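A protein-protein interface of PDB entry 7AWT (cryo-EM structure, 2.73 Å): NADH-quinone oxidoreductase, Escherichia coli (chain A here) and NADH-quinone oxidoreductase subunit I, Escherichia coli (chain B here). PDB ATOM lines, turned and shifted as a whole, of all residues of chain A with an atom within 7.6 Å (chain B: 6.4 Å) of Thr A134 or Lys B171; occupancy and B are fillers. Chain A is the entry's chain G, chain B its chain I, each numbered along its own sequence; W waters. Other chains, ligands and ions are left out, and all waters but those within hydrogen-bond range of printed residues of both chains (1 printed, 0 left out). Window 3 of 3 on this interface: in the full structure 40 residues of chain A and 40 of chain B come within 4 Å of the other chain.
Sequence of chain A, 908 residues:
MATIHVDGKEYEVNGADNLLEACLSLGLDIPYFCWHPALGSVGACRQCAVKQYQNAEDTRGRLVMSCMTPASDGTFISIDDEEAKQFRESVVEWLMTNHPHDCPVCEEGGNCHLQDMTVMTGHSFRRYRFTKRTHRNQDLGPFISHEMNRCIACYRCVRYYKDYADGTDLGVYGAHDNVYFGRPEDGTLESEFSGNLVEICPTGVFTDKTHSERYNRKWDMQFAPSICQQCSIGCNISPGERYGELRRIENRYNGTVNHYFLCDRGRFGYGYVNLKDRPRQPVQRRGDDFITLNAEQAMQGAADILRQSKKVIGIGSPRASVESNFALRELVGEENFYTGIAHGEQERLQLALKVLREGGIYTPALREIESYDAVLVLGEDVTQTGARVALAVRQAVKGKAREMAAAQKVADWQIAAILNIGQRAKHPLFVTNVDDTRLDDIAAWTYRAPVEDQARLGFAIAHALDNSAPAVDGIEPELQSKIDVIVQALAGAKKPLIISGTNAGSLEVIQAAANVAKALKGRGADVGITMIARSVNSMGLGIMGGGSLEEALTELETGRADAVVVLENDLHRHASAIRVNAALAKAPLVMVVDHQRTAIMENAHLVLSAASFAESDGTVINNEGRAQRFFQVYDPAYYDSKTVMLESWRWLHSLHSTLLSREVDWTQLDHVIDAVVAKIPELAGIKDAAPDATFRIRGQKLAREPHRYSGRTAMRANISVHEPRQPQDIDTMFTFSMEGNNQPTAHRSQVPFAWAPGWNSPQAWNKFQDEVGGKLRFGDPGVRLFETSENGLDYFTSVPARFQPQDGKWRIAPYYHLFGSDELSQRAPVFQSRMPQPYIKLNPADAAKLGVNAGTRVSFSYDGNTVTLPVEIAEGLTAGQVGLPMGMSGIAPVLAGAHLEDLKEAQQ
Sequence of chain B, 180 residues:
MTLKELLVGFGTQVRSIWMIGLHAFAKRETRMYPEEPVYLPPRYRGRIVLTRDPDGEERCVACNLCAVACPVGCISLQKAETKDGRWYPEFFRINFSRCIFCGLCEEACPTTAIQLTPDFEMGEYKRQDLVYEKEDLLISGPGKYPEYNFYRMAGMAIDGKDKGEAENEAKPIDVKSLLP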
ATOM      1  N   ASN A  98      -9.416   5.089   7.220  1.00  0.00           N
ATOM      2  CA  ASN A  98     -10.025   5.757   6.080  1.00  0.00           C
ATOM      3  C   ASN A  98      -9.519   7.138   5.730  1.00  0.00           C
ATOM      4  O   ASN A  98     -10.090   7.784   4.894  1.00  0.00           O
ATOM      5  CB  ASN A  98     -11.509   5.882   6.330  1.00  0.00           C
ATOM      6  CG  ASN A  98     -12.226   4.594   6.134  1.00  0.00           C
ATOM      7  OD1 ASN A  98     -11.898   3.816   5.261  1.00  0.00           O
ATOM      8  ND2 ASN A  98     -13.213   4.359   6.949  1.00  0.00           N
ATOM      9  N   PRO A 100      -7.313  10.269   4.179  1.00  0.00           N
ATOM     10  CA  PRO A 100      -6.680  10.656   2.942  1.00  0.00           C
ATOM     11  C   PRO A 100      -5.262  11.107   3.133  1.00  0.00           C
ATOM     12  O   PRO A 100      -5.020  11.953   3.914  1.00  0.00           O
ATOM     13  CB  PRO A 100      -7.533  11.807   2.522  1.00  0.00           C
ATOM     14  CG  PRO A 100      -7.953  12.409   3.749  1.00  0.00           C
ATOM     15  CD  PRO A 100      -8.268  11.273   4.601  1.00  0.00           C
ATOM     16  N   THR A 131      -8.583  -0.702   0.912  1.00  0.00           N
ATOM     17  CA  THR A 131      -8.957   0.576   0.339  1.00  0.00           C
ATOM     18  C   THR A 131      -9.614   1.475   1.380  1.00  0.00           C
ATOM     19  O   THR A 131     -10.125   1.018   2.404  1.00  0.00           O
ATOM     20  CB  THR A 131      -9.909   0.370  -0.836  1.00  0.00           C
ATOM     21  OG1 THR A 131     -11.004  -0.455  -0.420  1.00  0.00           O
ATOM     22  CG2 THR A 131      -9.190  -0.310  -1.984  1.00  0.00           C
ATOM     23  N   LYS A 132      -9.596   2.772   1.102  1.00  0.00           N
ATOM     24  CA  LYS A 132     -10.244   3.770   1.935  1.00  0.00           C
ATOM     25  C   LYS A 132     -11.528   4.240   1.267  1.00  0.00           C
ATOM     26  O   LYS A 132     -11.643   4.234   0.039  1.00  0.00           O
ATOM     27  CB  LYS A 132      -9.332   4.973   2.174  1.00  0.00           C
ATOM     28  CG  LYS A 132      -7.871   4.637   2.335  1.00  0.00           C
ATOM     29  CD  LYS A 132      -7.046   5.905   2.328  1.00  0.00           C
ATOM     30  CE  LYS A 132      -5.583   5.620   2.554  1.00  0.00           C
ATOM     31  NZ  LYS A 132      -4.834   6.871   2.821  1.00  0.00           N
ATOM     32  N   ARG A 133     -12.494   4.662   2.060  1.00  0.00           N
ATOM     33  CA  ARG A 133     -13.727   5.190   1.521  1.00  0.00           C
ATOM     34  C   ARG A 133     -13.470   6.621   1.101  1.00  0.00           C
ATOM     35  O   ARG A 133     -12.708   7.323   1.727  1.00  0.00           O
ATOM     36  CB  ARG A 133     -14.872   5.074   2.521  1.00  0.00           C
ATOM     37  CG  ARG A 133     -14.712   5.875   3.782  1.00  0.00           C
ATOM     38  CD  ARG A 133     -15.123   7.304   3.557  1.00  0.00           C
ATOM     39  NE  ARG A 133     -14.094   8.236   3.983  1.00  0.00           N
ATOM     40  CZ  ARG A 133     -14.185   9.008   5.044  1.00  0.00           C
ATOM     41  NH1 ARG A 133     -13.207   9.818   5.355  1.00  0.00           N
ATOM     42  NH2 ARG A 133     -15.261   8.972   5.783  1.00  0.00           N
ATOM     43  N   THR A 134     -14.110   7.048   0.031  1.00  0.00           N
ATOM     44  CA  THR A 134     -13.924   8.378  -0.519  1.00  0.00           C
ATOM     45  C   THR A 134     -15.273   9.049  -0.618  1.00  0.00           C
ATOM     46  O   THR A 134     -16.282   8.393  -0.590  1.00  0.00           O
ATOM     47  CB  THR A 134     -13.268   8.372  -1.894  1.00  0.00           C
ATOM     48  OG1 THR A 134     -14.052   7.626  -2.818  1.00  0.00           O
ATOM     49  CG2 THR A 134     -11.928   7.725  -1.811  1.00  0.00           C
ATOM     50  N   HIS A 135     -15.298  10.361  -0.711  1.00  0.00           N
ATOM     51  CA  HIS A 135     -16.535  11.119  -0.761  1.00  0.00           C
ATOM     52  C   HIS A 135     -16.363  12.291  -1.710  1.00  0.00           C
ATOM     53  O   HIS A 135     -15.264  12.826  -1.864  1.00  0.00           O
ATOM     54  CB  HIS A 135     -16.940  11.622   0.624  1.00  0.00           C
ATOM     55  CG  HIS A 135     -17.711  10.624   1.425  1.00  0.00           C
ATOM     56  ND1 HIS A 135     -18.894  10.072   0.986  1.00  0.00           N
ATOM     57  CD2 HIS A 135     -17.470  10.079   2.640  1.00  0.00           C
ATOM     58  CE1 HIS A 135     -19.347   9.228   1.893  1.00  0.00           C
ATOM     59  NE2 HIS A 135     -18.502   9.215   2.908  1.00  0.00           N
ATOM     60  N   ARG A 136     -17.472  12.732  -2.284  1.00  0.00           N
ATOM     61  CA  ARG A 136     -17.496  13.883  -3.162  1.00  0.00           C
ATOM     62  C   ARG A 136     -17.850  15.093  -2.332  1.00  0.00           C
ATOM     63  O   ARG A 136     -18.604  15.004  -1.391  1.00  0.00           O
ATOM     64  CB  ARG A 136     -18.498  13.702  -4.274  1.00  0.00           C
ATOM     65  CG  ARG A 136     -18.148  12.563  -5.185  1.00  0.00           C
ATOM     66  CD  ARG A 136     -18.746  12.757  -6.551  1.00  0.00           C
ATOM     67  NE  ARG A 136     -18.308  11.684  -7.420  1.00  0.00           N
ATOM     68  CZ  ARG A 136     -17.192  11.717  -8.127  1.00  0.00           C
ATOM     69  NH1 ARG A 136     -16.412  12.776  -8.082  1.00  0.00           N
ATOM     70  NH2 ARG A 136     -16.863  10.694  -8.884  1.00  0.00           N
ATOM     71  N   MET A 148     -15.022  16.133   2.397  1.00  0.00           N
ATOM     72  CA  MET A 148     -15.566  15.070   3.230  1.00  0.00           C
ATOM     73  C   MET A 148     -14.668  13.848   3.297  1.00  0.00           C
ATOM     74  O   MET A 148     -14.977  12.925   4.057  1.00  0.00           O
ATOM     75  CB  MET A 148     -16.948  14.664   2.731  1.00  0.00           C
ATOM     76  CG  MET A 148     -18.079  15.211   3.570  1.00  0.00           C
ATOM     77  SD  MET A 148     -18.078  14.571   5.247  1.00  0.00           S
ATOM     78  CE  MET A 148     -18.078  12.818   4.924  1.00  0.00           C
ATOM     79  N   ASN A 149     -13.580  13.799   2.530  1.00  0.00           N
ATOM     80  CA  ASN A 149     -12.653  12.685   2.662  1.00  0.00           C
ATOM     81  C   ASN A 149     -12.005  12.667   4.035  1.00  0.00           C
ATOM     82  O   ASN A 149     -11.640  11.599   4.537  1.00  0.00           O
ATOM     83  CB  ASN A 149     -11.581  12.758   1.579  1.00  0.00           C
ATOM     84  CG  ASN A 149     -11.957  11.992   0.341  1.00  0.00           C
ATOM     85  OD1 ASN A 149     -13.066  11.475   0.234  1.00  0.00           O
ATOM     86  ND2 ASN A 149     -11.039  11.918  -0.610  1.00  0.00           N
ATOM     87  N   ASP A 177     -20.573   3.656   8.228  1.00  0.00           N
ATOM     88  CA  ASP A 177     -19.204   3.923   7.793  1.00  0.00           C
ATOM     89  C   ASP A 177     -19.202   4.732   6.498  1.00  0.00           C
ATOM     90  O   ASP A 177     -18.161   5.230   6.064  1.00  0.00           O
ATOM     91  CB  ASP A 177     -18.450   2.589   7.637  1.00  0.00           C
ATOM     92  CG  ASP A 177     -17.162   2.718   6.864  1.00  0.00           C
ATOM     93  OD1 ASP A 177     -16.354   3.610   7.201  1.00  0.00           O
ATOM     94  OD2 ASP A 177     -16.960   1.930   5.917  1.00  0.00           O
ATOM     95  N   ASN A 178     -20.381   4.925   5.911  1.00  0.00           N
ATOM     96  CA  ASN A 178     -20.559   5.779   4.746  1.00  0.00           C
ATOM     97  C   ASN A 178     -21.271   7.072   5.119  1.00  0.00           C
ATOM     98  O   ASN A 178     -21.848   7.737   4.257  1.00  0.00           O
ATOM     99  CB  ASN A 178     -21.325   5.027   3.658  1.00  0.00           C
ATOM    100  CG  ASN A 178     -21.286   5.731   2.324  1.00  0.00           C
ATOM    101  OD1 ASN A 178     -22.300   6.237   1.851  1.00  0.00           O
ATOM    102  ND2 ASN A 178     -20.112   5.775   1.710  1.00  0.00           N
ATOM    103  N   TYR A 180     -22.253  10.882   6.175  1.00  0.00           N
ATOM    104  CA  TYR A 180     -21.927  12.084   5.418  1.00  0.00           C
ATOM    105  C   TYR A 180     -22.451  13.310   6.147  1.00  0.00           C
ATOM    106  O   TYR A 180     -23.567  13.293   6.672  1.00  0.00           O
ATOM    107  CB  TYR A 180     -22.529  12.014   4.014  1.00  0.00           C
ATOM    108  CG  TYR A 180     -21.984  13.003   3.014  1.00  0.00           C
ATOM    109  CD1 TYR A 180     -22.506  14.279   2.914  1.00  0.00           C
ATOM    110  CD2 TYR A 180     -20.970  12.644   2.144  1.00  0.00           C
ATOM    111  CE1 TYR A 180     -22.017  15.174   1.991  1.00  0.00           C
ATOM    112  CE2 TYR A 180     -20.477  13.536   1.224  1.00  0.00           C
ATOM    113  CZ  TYR A 180     -21.003  14.796   1.151  1.00  0.00           C
ATOM    114  OH  TYR A 180     -20.509  15.681   0.231  1.00  0.00           O
ATOM    115  N   GLY B 155      -5.575  12.517  -1.349  1.00  0.00           N
ATOM    116  CA  GLY B 155      -6.973  12.149  -1.407  1.00  0.00           C
ATOM    117  C   GLY B 155      -7.857  13.182  -2.070  1.00  0.00           C
ATOM    118  O   GLY B 155      -9.013  12.894  -2.392  1.00  0.00           O
ATOM    119  N   LYS B 163     -11.945  11.712  -7.431  1.00  0.00           N
ATOM    120  CA  LYS B 163     -12.013  11.408  -6.006  1.00  0.00           C
ATOM    121  C   LYS B 163     -11.638   9.960  -5.712  1.00  0.00           C
ATOM    122  O   LYS B 163     -10.987   9.678  -4.701  1.00  0.00           O
ATOM    123  CB  LYS B 163     -13.410  11.713  -5.473  1.00  0.00           C
ATOM    124  CG  LYS B 163     -13.577  13.131  -4.982  1.00  0.00           C
ATOM    125  CD  LYS B 163     -12.584  13.451  -3.885  1.00  0.00           C
ATOM    126  CE  LYS B 163     -12.697  14.900  -3.461  1.00  0.00           C
ATOM    127  NZ  LYS B 163     -11.789  15.226  -2.331  1.00  0.00           N
ATOM    128  N   GLY B 164     -12.032   9.031  -6.574  1.00  0.00           N
ATOM    129  CA  GLY B 164     -11.788   7.632  -6.288  1.00  0.00           C
ATOM    130  C   GLY B 164     -10.637   7.023  -7.056  1.00  0.00           C
ATOM    131  O   GLY B 164     -10.553   5.799  -7.183  1.00  0.00           O
ATOM    132  N   GLU B 165      -9.734   7.858  -7.567  1.00  0.00           N
ATOM    133  CA  GLU B 165      -8.663   7.397  -8.440  1.00  0.00           C
ATOM    134  C   GLU B 165      -7.284   7.492  -7.802  1.00  0.00           C
ATOM    135  O   GLU B 165      -6.279   7.364  -8.507  1.00  0.00           O
ATOM    136  CB  GLU B 165      -8.686   8.179  -9.753  1.00  0.00           C
ATOM    137  CG  GLU B 165      -9.756   7.715 -10.718  1.00  0.00           C
ATOM    138  CD  GLU B 165      -9.698   8.444 -12.040  1.00  0.00           C
ATOM    139  OE1 GLU B 165     -10.522   9.357 -12.253  1.00  0.00           O
ATOM    140  OE2 GLU B 165      -8.824   8.107 -12.866  1.00  0.00           O
ATOM    141  N   GLU B 169      -7.588   3.419  -2.900  1.00  0.00           N
ATOM    142  CA  GLU B 169      -8.803   4.159  -2.609  1.00  0.00           C
ATOM    143  C   GLU B 169      -9.965   3.518  -3.348  1.00  0.00           C
ATOM    144  O   GLU B 169      -9.787   2.901  -4.399  1.00  0.00           O
ATOM    145  CB  GLU B 169      -8.675   5.630  -3.005  1.00  0.00           C
ATOM    146  CG  GLU B 169      -7.987   6.476  -1.960  1.00  0.00           C
ATOM    147  CD  GLU B 169      -8.440   7.915  -1.991  1.00  0.00           C
ATOM    148  OE1 GLU B 169      -8.920   8.362  -3.052  1.00  0.00           O
ATOM    149  OE2 GLU B 169      -8.319   8.598  -0.953  1.00  0.00           O
ATOM    150  N   ALA B 170     -11.159   3.676  -2.788  1.00  0.00           N
ATOM    151  CA  ALA B 170     -12.368   3.087  -3.338  1.00  0.00           C
ATOM    152  C   ALA B 170     -13.227   4.161  -3.988  1.00  0.00           C
ATOM    153  O   ALA B 170     -13.136   5.342  -3.647  1.00  0.00           O
ATOM    154  CB  ALA B 170     -13.172   2.367  -2.255  1.00  0.00           C
ATOM    155  N   LYS B 171     -14.047   3.782  -4.955  1.00  0.00           N
ATOM    156  CA  LYS B 171     -14.888   4.763  -5.612  1.00  0.00           C
ATOM    157  C   LYS B 171     -15.893   5.258  -4.605  1.00  0.00           C
ATOM    158  O   LYS B 171     -16.410   4.472  -3.842  1.00  0.00           O
ATOM    159  CB  LYS B 171     -15.562   4.159  -6.824  1.00  0.00           C
ATOM    160  CG  LYS B 171     -14.574   3.830  -7.917  1.00  0.00           C
ATOM    161  CD  LYS B 171     -15.218   3.909  -9.284  1.00  0.00           C
ATOM    162  CE  LYS B 171     -14.157   4.009 -10.363  1.00  0.00           C
ATOM    163  NZ  LYS B 171     -14.739   3.934 -11.730  1.00  0.00           N
ATOM    164  N   PRO B 172     -16.199   6.554  -4.617  1.00  0.00           N
ATOM    165  CA  PRO B 172     -17.104   7.163  -3.634  1.00  0.00           C
ATOM    166  C   PRO B 172     -18.523   6.642  -3.800  1.00  0.00           C
ATOM    167  O   PRO B 172     -19.109   6.734  -4.881  1.00  0.00           O
ATOM    168  CB  PRO B 172     -17.011   8.659  -3.947  1.00  0.00           C
ATOM    169  CG  PRO B 172     -16.566   8.719  -5.352  1.00  0.00           C
ATOM    170  CD  PRO B 172     -15.657   7.551  -5.552  1.00  0.00           C
ATOM    171  N   ILE B 173     -19.069   6.087  -2.726  1.00  0.00           N
ATOM    172  CA  ILE B 173     -20.447   5.613  -2.708  1.00  0.00           C
ATOM    173  C   ILE B 173     -21.341   6.756  -2.254  1.00  0.00           C
ATOM    174  O   ILE B 173     -21.112   7.353  -1.197  1.00  0.00           O
ATOM    175  CB  ILE B 173     -20.599   4.396  -1.781  1.00  0.00           C
ATOM    176  CG1 ILE B 173     -19.765   3.227  -2.296  1.00  0.00           C
ATOM    177  CG2 ILE B 173     -22.054   3.994  -1.669  1.00  0.00           C
ATOM    178  CD1 ILE B 173     -19.843   2.004  -1.420  1.00  0.00           C
HETATM  179  O   HOH W   1     -10.103   8.941   1.428  1.00  0.00           O
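O of Lys A132 is in hydrogen-bond range of N of Ala B170, at 2.9 Å. The backbone carbonyl oxygen (O) of Ala B170 sits at hydrogen-bond distance from the side-chain hydroxyl (OG1) of Thr A134, 2.6 Å away. The backbone carbonyl oxygen (O) of Gly B155 lies within hydrogen-bond range of the side-chain amide nitrogen (ND2) of Asn A149, 2.9 Å away. O of Ile B173 is in hydrogen-bond range of ND2 of Asn A178, at 3.5 Å. OG1 of Thr A134 sits close to N of Pro B172, 3.0 Å away.
The guanidinium group (NH1) of Arg A133 sits at hydrogen-bond distance from the backbone carbonyl oxygen (O) of Asn A149 (2.5 Å). The side-chain amide oxygen (OD1) of Asn A149 is in hydrogen-bond range of the backbone NH (N) of His A135, at 2.7 Å.
Pro A100 touches Gly B155. Lys A132 touches Glu B169 (O to C, 3.8 Å). O of Lys B163 touches CG2 of Thr A134, 3.6 Å away. Glu B169 touches Thr A134 (OE1 to CG2, 3.3 Å). Lys B171 touches Thr A134. O of His A135 touches CD of Lys B163, 3.4 Å away. Lys B163 touches Asn A149.
Of the printed residues of chain B, Thr A134 touches Lys B163, Glu B169, Ala B170, Lys B171 and Pro B172. Of chain A, only Thr A134 comes within 4 Å of Lys B171. Of the printed residues of chain B, His A135 touches Lys B163. Of the printed residues of chain A, Ile B173 touches Asn A178 (3.5 Å). Printed residues of chain B within 4 Å of Asn A178: Ile B173 (3.5 Å). Printed residues of chain A within 4 Å of Lys B163: Thr A134 (3.6 Å), His A135 (3.4 Å) and Asn A149 (3.8 Å). Printed residues of chain B within 4 Å of Asn A149: Gly B155 and Lys B163. The nearest residue of chain B that does not touch Thr A134 is Gly B164 (4.1 Å). The nearest residue of chain A that does not touch Lys B171 is Lys A132 (5.6 Å). The nearest printed residue of chain B that does not touch Asn A178 is Pro B172 (5.8 Å).
Printed residues of chain B that touch a printed residue of chain A: Gly B155, Lys B163, Glu B169, Ala B170, Lys B171, Pro B172 and Ile B173. Hydrophobic or aromatic side chains of chain B within 4 Å of the printed part of chain A: Ala B170, Pro B172 and Ile B173. Hydrophobic or aromatic side chains of chain A within 4 Å of the printed part of chain B: Pro A100.
Water W1 bridges the side-chain carboxylate (OE2) of Glu B169 (3.0 Å) and the backbone carbonyl oxygen (O) of Arg A133 (3.1 Å).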
